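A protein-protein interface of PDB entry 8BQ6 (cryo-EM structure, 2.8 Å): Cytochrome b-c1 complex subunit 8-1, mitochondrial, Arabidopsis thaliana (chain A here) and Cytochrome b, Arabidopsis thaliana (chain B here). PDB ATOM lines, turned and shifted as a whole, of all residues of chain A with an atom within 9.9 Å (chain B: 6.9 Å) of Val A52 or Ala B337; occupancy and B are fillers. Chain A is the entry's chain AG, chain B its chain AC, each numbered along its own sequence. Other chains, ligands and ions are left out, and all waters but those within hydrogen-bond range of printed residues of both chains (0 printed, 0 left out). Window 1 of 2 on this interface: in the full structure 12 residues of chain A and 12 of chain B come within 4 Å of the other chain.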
ATOM      1  N   SER A  44     -33.535  18.510  17.218  1.00  0.00           N
ATOM      2  CA  SER A  44     -32.173  18.861  17.609  1.00  0.00           C
ATOM      3  C   SER A  44     -31.447  17.669  18.218  1.00  0.00           C
ATOM      4  O   SER A  44     -30.239  17.496  18.021  1.00  0.00           O
ATOM      5  CB  SER A  44     -32.194  20.027  18.593  1.00  0.00           C
ATOM      6  OG  SER A  44     -32.609  21.221  17.960  1.00  0.00           O
ATOM      7  N   ALA A  45     -32.162  16.851  18.992  1.00  0.00           N
ATOM      8  CA  ALA A  45     -31.526  15.692  19.607  1.00  0.00           C
ATOM      9  C   ALA A  45     -31.199  14.630  18.566  1.00  0.00           C
ATOM     10  O   ALA A  45     -30.233  13.874  18.721  1.00  0.00           O
ATOM     11  CB  ALA A  45     -32.424  15.118  20.702  1.00  0.00           C
ATOM     12  N   THR A  46     -31.993  14.558  17.498  1.00  0.00           N
ATOM     13  CA  THR A  46     -31.724  13.593  16.437  1.00  0.00           C
ATOM     14  C   THR A  46     -30.520  14.020  15.606  1.00  0.00           C
ATOM     15  O   THR A  46     -29.710  13.187  15.186  1.00  0.00           O
ATOM     16  CB  THR A  46     -32.968  13.426  15.564  1.00  0.00           C
ATOM     17  OG1 THR A  46     -33.970  12.717  16.302  1.00  0.00           O
ATOM     18  CG2 THR A  46     -32.647  12.641  14.311  1.00  0.00           C
ATOM     19  N   LEU A  47     -30.372  15.326  15.376  1.00  0.00           N
ATOM     20  CA  LEU A  47     -29.228  15.802  14.609  1.00  0.00           C
ATOM     21  C   LEU A  47     -27.935  15.736  15.415  1.00  0.00           C
ATOM     22  O   LEU A  47     -26.849  15.898  14.849  1.00  0.00           O
ATOM     23  CB  LEU A  47     -29.480  17.226  14.114  1.00  0.00           C
ATOM     24  CG  LEU A  47     -30.658  17.434  13.160  1.00  0.00           C
ATOM     25  CD1 LEU A  47     -30.981  18.912  13.039  1.00  0.00           C
ATOM     26  CD2 LEU A  47     -30.350  16.849  11.799  1.00  0.00           C
ATOM     27  N   LEU A  48     -28.018  15.496  16.725  1.00  0.00           N
ATOM     28  CA  LEU A  48     -26.796  15.363  17.513  1.00  0.00           C
ATOM     29  C   LEU A  48     -26.472  13.903  17.805  1.00  0.00           C
ATOM     30  O   LEU A  48     -25.296  13.526  17.872  1.00  0.00           O
ATOM     31  CB  LEU A  48     -26.911  16.158  18.817  1.00  0.00           C
ATOM     32  CG  LEU A  48     -25.851  15.878  19.890  1.00  0.00           C
ATOM     33  CD1 LEU A  48     -24.505  16.411  19.443  1.00  0.00           C
ATOM     34  CD2 LEU A  48     -26.234  16.477  21.236  1.00  0.00           C
ATOM     35  N   VAL A  49     -27.493  13.066  17.960  1.00  0.00           N
ATOM     36  CA  VAL A  49     -27.292  11.688  18.396  1.00  0.00           C
ATOM     37  C   VAL A  49     -27.105  10.741  17.216  1.00  0.00           C
ATOM     38  O   VAL A  49     -26.289   9.818  17.280  1.00  0.00           O
ATOM     39  CB  VAL A  49     -28.470  11.264  19.299  1.00  0.00           C
ATOM     40  CG1 VAL A  49     -28.719   9.769  19.229  1.00  0.00           C
ATOM     41  CG2 VAL A  49     -28.198  11.683  20.727  1.00  0.00           C
ATOM     42  N   THR A  50     -27.834  10.963  16.122  1.00  0.00           N
ATOM     43  CA  THR A  50     -27.755  10.060  14.973  1.00  0.00           C
ATOM     44  C   THR A  50     -26.363   9.983  14.353  1.00  0.00           C
ATOM     45  O   THR A  50     -25.893   8.861  14.100  1.00  0.00           O
ATOM     46  CB  THR A  50     -28.803  10.465  13.930  1.00  0.00           C
ATOM     47  OG1 THR A  50     -30.088  10.559  14.556  1.00  0.00           O
ATOM     48  CG2 THR A  50     -28.868   9.448  12.806  1.00  0.00           C
ATOM     49  N   PRO A  51     -25.665  11.091  14.059  1.00  0.00           N
ATOM     50  CA  PRO A  51     -24.324  10.944  13.468  1.00  0.00           C
ATOM     51  C   PRO A  51     -23.331  10.253  14.383  1.00  0.00           C
ATOM     52  O   PRO A  51     -22.527   9.441  13.912  1.00  0.00           O
ATOM     53  CB  PRO A  51     -23.910  12.394  13.175  1.00  0.00           C
ATOM     54  CG  PRO A  51     -25.175  13.148  13.121  1.00  0.00           C
ATOM     55  CD  PRO A  51     -26.056  12.509  14.137  1.00  0.00           C
ATOM     56  N   VAL A  52     -23.365  10.553  15.684  1.00  0.00           N
ATOM     57  CA  VAL A  52     -22.439   9.923  16.622  1.00  0.00           C
ATOM     58  C   VAL A  52     -22.686   8.423  16.688  1.00  0.00           C
ATOM     59  O   VAL A  52     -21.761   7.615  16.548  1.00  0.00           O
ATOM     60  CB  VAL A  52     -22.560  10.568  18.013  1.00  0.00           C
ATOM     61  CG1 VAL A  52     -21.704   9.816  19.014  1.00  0.00           C
ATOM     62  CG2 VAL A  52     -22.151  12.021  17.962  1.00  0.00           C
ATOM     63  N   VAL A  53     -23.940   8.027  16.899  1.00  0.00           N
ATOM     64  CA  VAL A  53     -24.257   6.609  17.032  1.00  0.00           C
ATOM     65  C   VAL A  53     -24.115   5.897  15.692  1.00  0.00           C
ATOM     66  O   VAL A  53     -23.627   4.763  15.627  1.00  0.00           O
ATOM     67  CB  VAL A  53     -25.662   6.440  17.635  1.00  0.00           C
ATOM     68  CG1 VAL A  53     -26.126   5.005  17.520  1.00  0.00           C
ATOM     69  CG2 VAL A  53     -25.648   6.866  19.094  1.00  0.00           C
ATOM     70  N   GLY A  54     -24.528   6.549  14.604  1.00  0.00           N
ATOM     71  CA  GLY A  54     -24.413   5.924  13.295  1.00  0.00           C
ATOM     72  C   GLY A  54     -22.974   5.688  12.879  1.00  0.00           C
ATOM     73  O   GLY A  54     -22.628   4.618  12.376  1.00  0.00           O
ATOM     74  N   THR A  55     -22.116   6.691  13.070  1.00  0.00           N
ATOM     75  CA  THR A  55     -20.714   6.527  12.696  1.00  0.00           C
ATOM     76  C   THR A  55     -20.020   5.508  13.591  1.00  0.00           C
ATOM     77  O   THR A  55     -19.216   4.700  13.112  1.00  0.00           O
ATOM     78  CB  THR A  55     -19.997   7.874  12.740  1.00  0.00           C
ATOM     79  OG1 THR A  55     -20.744   8.829  11.978  1.00  0.00           O
ATOM     80  CG2 THR A  55     -18.609   7.755  12.155  1.00  0.00           C
ATOM     81  N   TYR A  56     -20.331   5.521  14.886  1.00  0.00           N
ATOM     82  CA  TYR A  56     -19.770   4.534  15.801  1.00  0.00           C
ATOM     83  C   TYR A  56     -20.197   3.121  15.422  1.00  0.00           C
ATOM     84  O   TYR A  56     -19.385   2.190  15.435  1.00  0.00           O
ATOM     85  CB  TYR A  56     -20.199   4.861  17.228  1.00  0.00           C
ATOM     86  CG  TYR A  56     -19.585   3.979  18.278  1.00  0.00           C
ATOM     87  CD1 TYR A  56     -18.345   4.280  18.821  1.00  0.00           C
ATOM     88  CD2 TYR A  56     -20.246   2.849  18.733  1.00  0.00           C
ATOM     89  CE1 TYR A  56     -17.784   3.483  19.782  1.00  0.00           C
ATOM     90  CE2 TYR A  56     -19.691   2.046  19.695  1.00  0.00           C
ATOM     91  CZ  TYR A  56     -18.457   2.364  20.216  1.00  0.00           C
ATOM     92  OH  TYR A  56     -17.894   1.563  21.181  1.00  0.00           O
ATOM     93  N   TRP A  57     -21.479   2.941  15.086  1.00  0.00           N
ATOM     94  CA  TRP A  57     -21.974   1.609  14.749  1.00  0.00           C
ATOM     95  C   TRP A  57     -21.330   1.082  13.478  1.00  0.00           C
ATOM     96  O   TRP A  57     -21.062  -0.119  13.361  1.00  0.00           O
ATOM     97  CB  TRP A  57     -23.494   1.624  14.602  1.00  0.00           C
ATOM     98  CG  TRP A  57     -24.124   0.333  14.996  1.00  0.00           C
ATOM     99  CD1 TRP A  57     -23.774  -0.917  14.575  1.00  0.00           C
ATOM    100  CD2 TRP A  57     -25.182   0.157  15.943  1.00  0.00           C
ATOM    101  NE1 TRP A  57     -24.569  -1.859  15.181  1.00  0.00           N
ATOM    102  CE2 TRP A  57     -25.439  -1.225  16.029  1.00  0.00           C
ATOM    103  CE3 TRP A  57     -25.942   1.035  16.720  1.00  0.00           C
ATOM    104  CZ2 TRP A  57     -26.427  -1.749  16.859  1.00  0.00           C
ATOM    105  CZ3 TRP A  57     -26.922   0.513  17.542  1.00  0.00           C
ATOM    106  CH2 TRP A  57     -27.156  -0.866  17.607  1.00  0.00           C
ATOM    107  N   TYR A  58     -21.106   1.957  12.499  1.00  0.00           N
ATOM    108  CA  TYR A  58     -20.452   1.522  11.273  1.00  0.00           C
ATOM    109  C   TYR A  58     -19.009   1.110  11.537  1.00  0.00           C
ATOM    110  O   TYR A  58     -18.514   0.145  10.945  1.00  0.00           O
ATOM    111  CB  TYR A  58     -20.521   2.627  10.219  1.00  0.00           C
ATOM    112  CG  TYR A  58     -19.641   2.375   9.020  1.00  0.00           C
ATOM    113  CD1 TYR A  58     -20.118   1.672   7.927  1.00  0.00           C
ATOM    114  CD2 TYR A  58     -18.341   2.860   8.971  1.00  0.00           C
ATOM    115  CE1 TYR A  58     -19.322   1.440   6.828  1.00  0.00           C
ATOM    116  CE2 TYR A  58     -17.537   2.632   7.877  1.00  0.00           C
ATOM    117  CZ  TYR A  58     -18.034   1.923   6.806  1.00  0.00           C
ATOM    118  OH  TYR A  58     -17.240   1.695   5.707  1.00  0.00           O
ATOM    119  N   ALA A  59     -18.313   1.840  12.412  1.00  0.00           N
ATOM    120  CA  ALA A  59     -16.916   1.522  12.687  1.00  0.00           C
ATOM    121  C   ALA A  59     -16.779   0.159  13.358  1.00  0.00           C
ATOM    122  O   ALA A  59     -15.852  -0.597  13.051  1.00  0.00           O
ATOM    123  CB  ALA A  59     -16.283   2.615  13.544  1.00  0.00           C
ATOM    124  N   GLN A  60     -17.682  -0.166  14.285  1.00  0.00           N
ATOM    125  CA  GLN A  60     -17.689  -1.506  14.866  1.00  0.00           C
ATOM    126  C   GLN A  60     -18.081  -2.552  13.833  1.00  0.00           C
ATOM    127  O   GLN A  60     -17.568  -3.676  13.844  1.00  0.00           O
ATOM    128  CB  GLN A  60     -18.637  -1.560  16.064  1.00  0.00           C
ATOM    129  CG  GLN A  60     -17.954  -1.518  17.424  1.00  0.00           C
ATOM    130  CD  GLN A  60     -17.131  -0.267  17.645  1.00  0.00           C
ATOM    131  OE1 GLN A  60     -17.609   0.848  17.448  1.00  0.00           O
ATOM    132  NE2 GLN A  60     -15.888  -0.447  18.073  1.00  0.00           N
ATOM    133  N   PHE B 104     -19.297  26.899  22.675  1.00  0.00           N
ATOM    134  CA  PHE B 104     -20.454  26.466  21.904  1.00  0.00           C
ATOM    135  C   PHE B 104     -21.707  27.247  22.277  1.00  0.00           C
ATOM    136  O   PHE B 104     -22.633  27.350  21.465  1.00  0.00           O
ATOM    137  CB  PHE B 104     -20.653  24.964  22.075  1.00  0.00           C
ATOM    138  CG  PHE B 104     -19.791  24.151  21.159  1.00  0.00           C
ATOM    139  CD1 PHE B 104     -20.256  23.773  19.915  1.00  0.00           C
ATOM    140  CD2 PHE B 104     -18.506  23.794  21.526  1.00  0.00           C
ATOM    141  CE1 PHE B 104     -19.467  23.040  19.058  1.00  0.00           C
ATOM    142  CE2 PHE B 104     -17.711  23.060  20.673  1.00  0.00           C
ATOM    143  CZ  PHE B 104     -18.194  22.683  19.436  1.00  0.00           C
ATOM    144  N   PHE B 332     -25.831  23.839  13.804  1.00  0.00           N
ATOM    145  CA  PHE B 332     -25.034  23.891  15.024  1.00  0.00           C
ATOM    146  C   PHE B 332     -24.932  22.518  15.675  1.00  0.00           C
ATOM    147  O   PHE B 332     -23.853  22.112  16.122  1.00  0.00           O
ATOM    148  CB  PHE B 332     -25.628  24.907  16.002  1.00  0.00           C
ATOM    149  CG  PHE B 332     -25.134  24.751  17.413  1.00  0.00           C
ATOM    150  CD1 PHE B 332     -25.813  23.954  18.320  1.00  0.00           C
ATOM    151  CD2 PHE B 332     -23.983  25.396  17.830  1.00  0.00           C
ATOM    152  CE1 PHE B 332     -25.353  23.805  19.609  1.00  0.00           C
ATOM    153  CE2 PHE B 332     -23.523  25.252  19.120  1.00  0.00           C
ATOM    154  CZ  PHE B 332     -24.207  24.455  20.010  1.00  0.00           C
ATOM    155  N   TRP B 333     -26.048  21.788  15.737  1.00  0.00           N
ATOM    156  CA  TRP B 333     -26.048  20.476  16.376  1.00  0.00           C
ATOM    157  C   TRP B 333     -25.281  19.455  15.547  1.00  0.00           C
ATOM    158  O   TRP B 333     -24.693  18.516  16.097  1.00  0.00           O
ATOM    159  CB  TRP B 333     -27.484  20.017  16.622  1.00  0.00           C
ATOM    160  CG  TRP B 333     -28.190  20.852  17.642  1.00  0.00           C
ATOM    161  CD1 TRP B 333     -29.246  21.685  17.428  1.00  0.00           C
ATOM    162  CD2 TRP B 333     -27.890  20.935  19.041  1.00  0.00           C
ATOM    163  NE1 TRP B 333     -29.620  22.285  18.604  1.00  0.00           N
ATOM    164  CE2 TRP B 333     -28.804  21.839  19.610  1.00  0.00           C
ATOM    165  CE3 TRP B 333     -26.936  20.332  19.866  1.00  0.00           C
ATOM    166  CZ2 TRP B 333     -28.794  22.158  20.966  1.00  0.00           C
ATOM    167  CZ3 TRP B 333     -26.930  20.648  21.213  1.00  0.00           C
ATOM    168  CH2 TRP B 333     -27.852  21.552  21.749  1.00  0.00           C
ATOM    169  N   LEU B 334     -25.282  19.612  14.222  1.00  0.00           N
ATOM    170  CA  LEU B 334     -24.437  18.771  13.381  1.00  0.00           C
ATOM    171  C   LEU B 334     -22.959  19.076  13.602  1.00  0.00           C
ATOM    172  O   LEU B 334     -22.125  18.165  13.602  1.00  0.00           O
ATOM    173  CB  LEU B 334     -24.813  18.951  11.912  1.00  0.00           C
ATOM    174  CG  LEU B 334     -26.177  18.395  11.503  1.00  0.00           C
ATOM    175  CD1 LEU B 334     -26.519  18.811  10.083  1.00  0.00           C
ATOM    176  CD2 LEU B 334     -26.189  16.884  11.641  1.00  0.00           C
ATOM    177  N   LEU B 335     -22.615  20.354  13.781  1.00  0.00           N
ATOM    178  CA  LEU B 335     -21.236  20.714  14.104  1.00  0.00           C
ATOM    179  C   LEU B 335     -20.817  20.135  15.448  1.00  0.00           C
ATOM    180  O   LEU B 335     -19.686  19.658  15.604  1.00  0.00           O
ATOM    181  CB  LEU B 335     -21.072  22.233  14.111  1.00  0.00           C
ATOM    182  CG  LEU B 335     -19.748  22.779  14.664  1.00  0.00           C
ATOM    183  CD1 LEU B 335     -18.600  22.622  13.676  1.00  0.00           C
ATOM    184  CD2 LEU B 335     -19.890  24.221  15.123  1.00  0.00           C
ATOM    185  N   LEU B 336     -21.711  20.182  16.437  1.00  0.00           N
ATOM    186  CA  LEU B 336     -21.400  19.630  17.750  1.00  0.00           C
ATOM    187  C   LEU B 336     -21.162  18.128  17.673  1.00  0.00           C
ATOM    188  O   LEU B 336     -20.237  17.601  18.301  1.00  0.00           O
ATOM    189  CB  LEU B 336     -22.528  19.942  18.729  1.00  0.00           C
ATOM    190  CG  LEU B 336     -22.318  19.481  20.170  1.00  0.00           C
ATOM    191  CD1 LEU B 336     -21.002  19.987  20.729  1.00  0.00           C
ATOM    192  CD2 LEU B 336     -23.476  19.932  21.026  1.00  0.00           C
ATOM    193  N   ALA B 337     -22.001  17.418  16.916  1.00  0.00           N
ATOM    194  CA  ALA B 337     -21.803  15.986  16.730  1.00  0.00           C
ATOM    195  C   ALA B 337     -20.514  15.704  15.971  1.00  0.00           C
ATOM    196  O   ALA B 337     -19.783  14.760  16.292  1.00  0.00           O
ATOM    197  CB  ALA B 337     -22.999  15.382  15.995  1.00  0.00           C
ATOM    198  N   ASP B 338     -20.225  16.514  14.954  1.00  0.00           N
ATOM    199  CA  ASP B 338     -18.995  16.353  14.190  1.00  0.00           C
ATOM    200  C   ASP B 338     -17.764  16.583  15.061  1.00  0.00           C
ATOM    201  O   ASP B 338     -16.748  15.896  14.907  1.00  0.00           O
ATOM    202  CB  ASP B 338     -19.014  17.309  13.003  1.00  0.00           C
ATOM    203  CG  ASP B 338     -17.996  16.954  11.954  1.00  0.00           C
ATOM    204  OD1 ASP B 338     -18.258  16.048  11.139  1.00  0.00           O
ATOM    205  OD2 ASP B 338     -16.929  17.593  11.945  1.00  0.00           O
ATOM    206  N   CYS B 339     -17.831  17.561  15.970  1.00  0.00           N
ATOM    207  CA  CYS B 339     -16.708  17.820  16.869  1.00  0.00           C
ATOM    208  C   CYS B 339     -16.509  16.677  17.858  1.00  0.00           C
ATOM    209  O   CYS B 339     -15.370  16.344  18.206  1.00  0.00           O
ATOM    210  CB  CYS B 339     -16.920  19.138  17.611  1.00  0.00           C
ATOM    211  SG  CYS B 339     -16.684  20.610  16.597  1.00  0.00           S
ATOM    212  N   LEU B 340     -17.600  16.082  18.343  1.00  0.00           N
ATOM    213  CA  LEU B 340     -17.472  14.898  19.187  1.00  0.00           C
ATOM    214  C   LEU B 340     -16.886  13.734  18.399  1.00  0.00           C
ATOM    215  O   LEU B 340     -16.086  12.953  18.926  1.00  0.00           O
ATOM    216  CB  LEU B 340     -18.831  14.520  19.773  1.00  0.00           C
ATOM    217  CG  LEU B 340     -19.458  15.515  20.753  1.00  0.00           C
ATOM    218  CD1 LEU B 340     -20.851  15.062  21.160  1.00  0.00           C
ATOM    219  CD2 LEU B 340     -18.575  15.726  21.971  1.00  0.00           C
ATOM    220  N   LEU B 341     -17.284  13.601  17.130  1.00  0.00           N
ATOM    221  CA  LEU B 341     -16.761  12.537  16.280  1.00  0.00           C
ATOM    222  C   LEU B 341     -15.277  12.719  15.996  1.00  0.00           C
ATOM    223  O   LEU B 341     -14.526  11.739  15.933  1.00  0.00           O
ATOM    224  CB  LEU B 341     -17.541  12.494  14.970  1.00  0.00           C
ATOM    225  CG  LEU B 341     -18.774  11.602  14.937  1.00  0.00           C
ATOM    226  CD1 LEU B 341     -19.197  11.392  13.499  1.00  0.00           C
ATOM    227  CD2 LEU B 341     -18.469  10.279  15.606  1.00  0.00           C
ATOM    228  N   LEU B 342     -14.841  13.962  15.783  1.00  0.00           N
ATOM    229  CA  LEU B 342     -13.426  14.209  15.530  1.00  0.00           C
ATOM    230  C   LEU B 342     -12.579  13.846  16.742  1.00  0.00           C
ATOM    231  O   LEU B 342     -11.486  13.287  16.598  1.00  0.00           O
ATOM    232  CB  LEU B 342     -13.206  15.670  15.147  1.00  0.00           C
ATOM    233  CG  LEU B 342     -13.456  16.041  13.689  1.00  0.00           C
ATOM    234  CD1 LEU B 342     -13.563  17.546  13.566  1.00  0.00           C
ATOM    235  CD2 LEU B 342     -12.358  15.497  12.786  1.00  0.00           C
ATOM    236  N   TRP B 344     -13.261  11.562  18.956  1.00  0.00           N
ATOM    237  CA  TRP B 344     -13.211  10.106  19.035  1.00  0.00           C
ATOM    238  C   TRP B 344     -12.272   9.528  17.983  1.00  0.00           C
ATOM    239  O   TRP B 344     -11.580   8.536  18.237  1.00  0.00           O
ATOM    240  CB  TRP B 344     -14.624   9.538  18.888  1.00  0.00           C
ATOM    241  CG  TRP B 344     -14.690   8.059  18.702  1.00  0.00           C
ATOM    242  CD1 TRP B 344     -14.435   7.099  19.636  1.00  0.00           C
ATOM    243  CD2 TRP B 344     -15.052   7.368  17.504  1.00  0.00           C
ATOM    244  NE1 TRP B 344     -14.608   5.851  19.090  1.00  0.00           N
ATOM    245  CE2 TRP B 344     -14.988   5.990  17.781  1.00  0.00           C
ATOM    246  CE3 TRP B 344     -15.421   7.781  16.223  1.00  0.00           C
ATOM    247  CZ2 TRP B 344     -15.279   5.025  16.825  1.00  0.00           C
ATOM    248  CZ3 TRP B 344     -15.708   6.823  15.277  1.00  0.00           C
ATOM    249  CH2 TRP B 344     -15.637   5.461  15.581  1.00  0.00           C
ATOM    250  N   SER B 361     -15.148  13.959   8.524  1.00  0.00           N
ATOM    251  CA  SER B 361     -15.412  14.783   9.700  1.00  0.00           C
ATOM    252  C   SER B 361     -14.667  16.111   9.629  1.00  0.00           C
ATOM    253  O   SER B 361     -15.200  17.151  10.030  1.00  0.00           O
ATOM    254  CB  SER B 361     -15.029  14.025  10.969  1.00  0.00           C
ATOM    255  OG  SER B 361     -15.964  13.004  11.256  1.00  0.00           O
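The side-chain hydroxyl of Ser A44 lies within hydrogen-bond range of the indole nitrogen of Trp B333, at 3.2 Å.
The side-chain hydroxyl (OG1) of Thr A55 sits at hydrogen-bond distance from the backbone carbonyl oxygen (O) of Pro A51, at 2.7 Å. The backbone carbonyl oxygen (O) of Tyr A56 lies close to the side-chain amide oxygen (OE1) of Gln A60.
O of Leu A47 touches O of Trp B333 (3.6 Å). Leu A47 touches Leu B334 (O to CD2, 3.4 Å). CD1 of Leu A48 touches O of Trp B333 (3.96 Å). Leu B336 touches Leu A48 (CG to CD1, 3.8 Å). Leu A48 touches Ala B337. Pro A51 touches Leu B341. Val A52 touches Ala B337. Thr A55 touches Leu B341 (OG1 to CD1, 3.4 Å). CD1 of Tyr A56 touches CZ2 of Trp B344 (3.7 Å). Trp B344 touches Ala A59.
Of the printed residues of chain B, Val A52 touches Ala B337. Printed residues of chain A within 4 Å of Ala B337: Leu A48 (3.5 Å) and Val A52 (3.99 Å). Leu B336 touches just one residue of chain A: Leu A48. No residue of chain A comes within 4 Å of Asp B338. Of the printed residues of chain B, Thr A55 touches Leu B341. Printed residues of chain A within 4 Å of Leu B334: Leu A47. Phe B104 touches none of the printed residues of chain A. The nearest printed residue of chain B that does not touch Val A52 is Leu B341 (4.1 Å). The nearest printed residue of chain A that does not touch Ala B337 is Leu A47 (4.05 Å). The nearest printed residue of chain A that does not touch Trp B333 is Ala A45 (5.8 Å).
Printed residues of chain A that touch a printed residue of chain B: Ser A44, Leu A47, Leu A48, Pro A51, Val A52, Thr A55, Tyr A56 and Ala A59. Hydrophobic or aromatic side chains of chain A that line the printed part of chain B: Leu A48, Val A52, Tyr A56 and Ala A59. Hydrophobic or aromatic side chains of chain B that line the printed part of chain A: Trp B333, Leu B334, Leu B336, Ala B337, Leu B341 and Trp B344.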
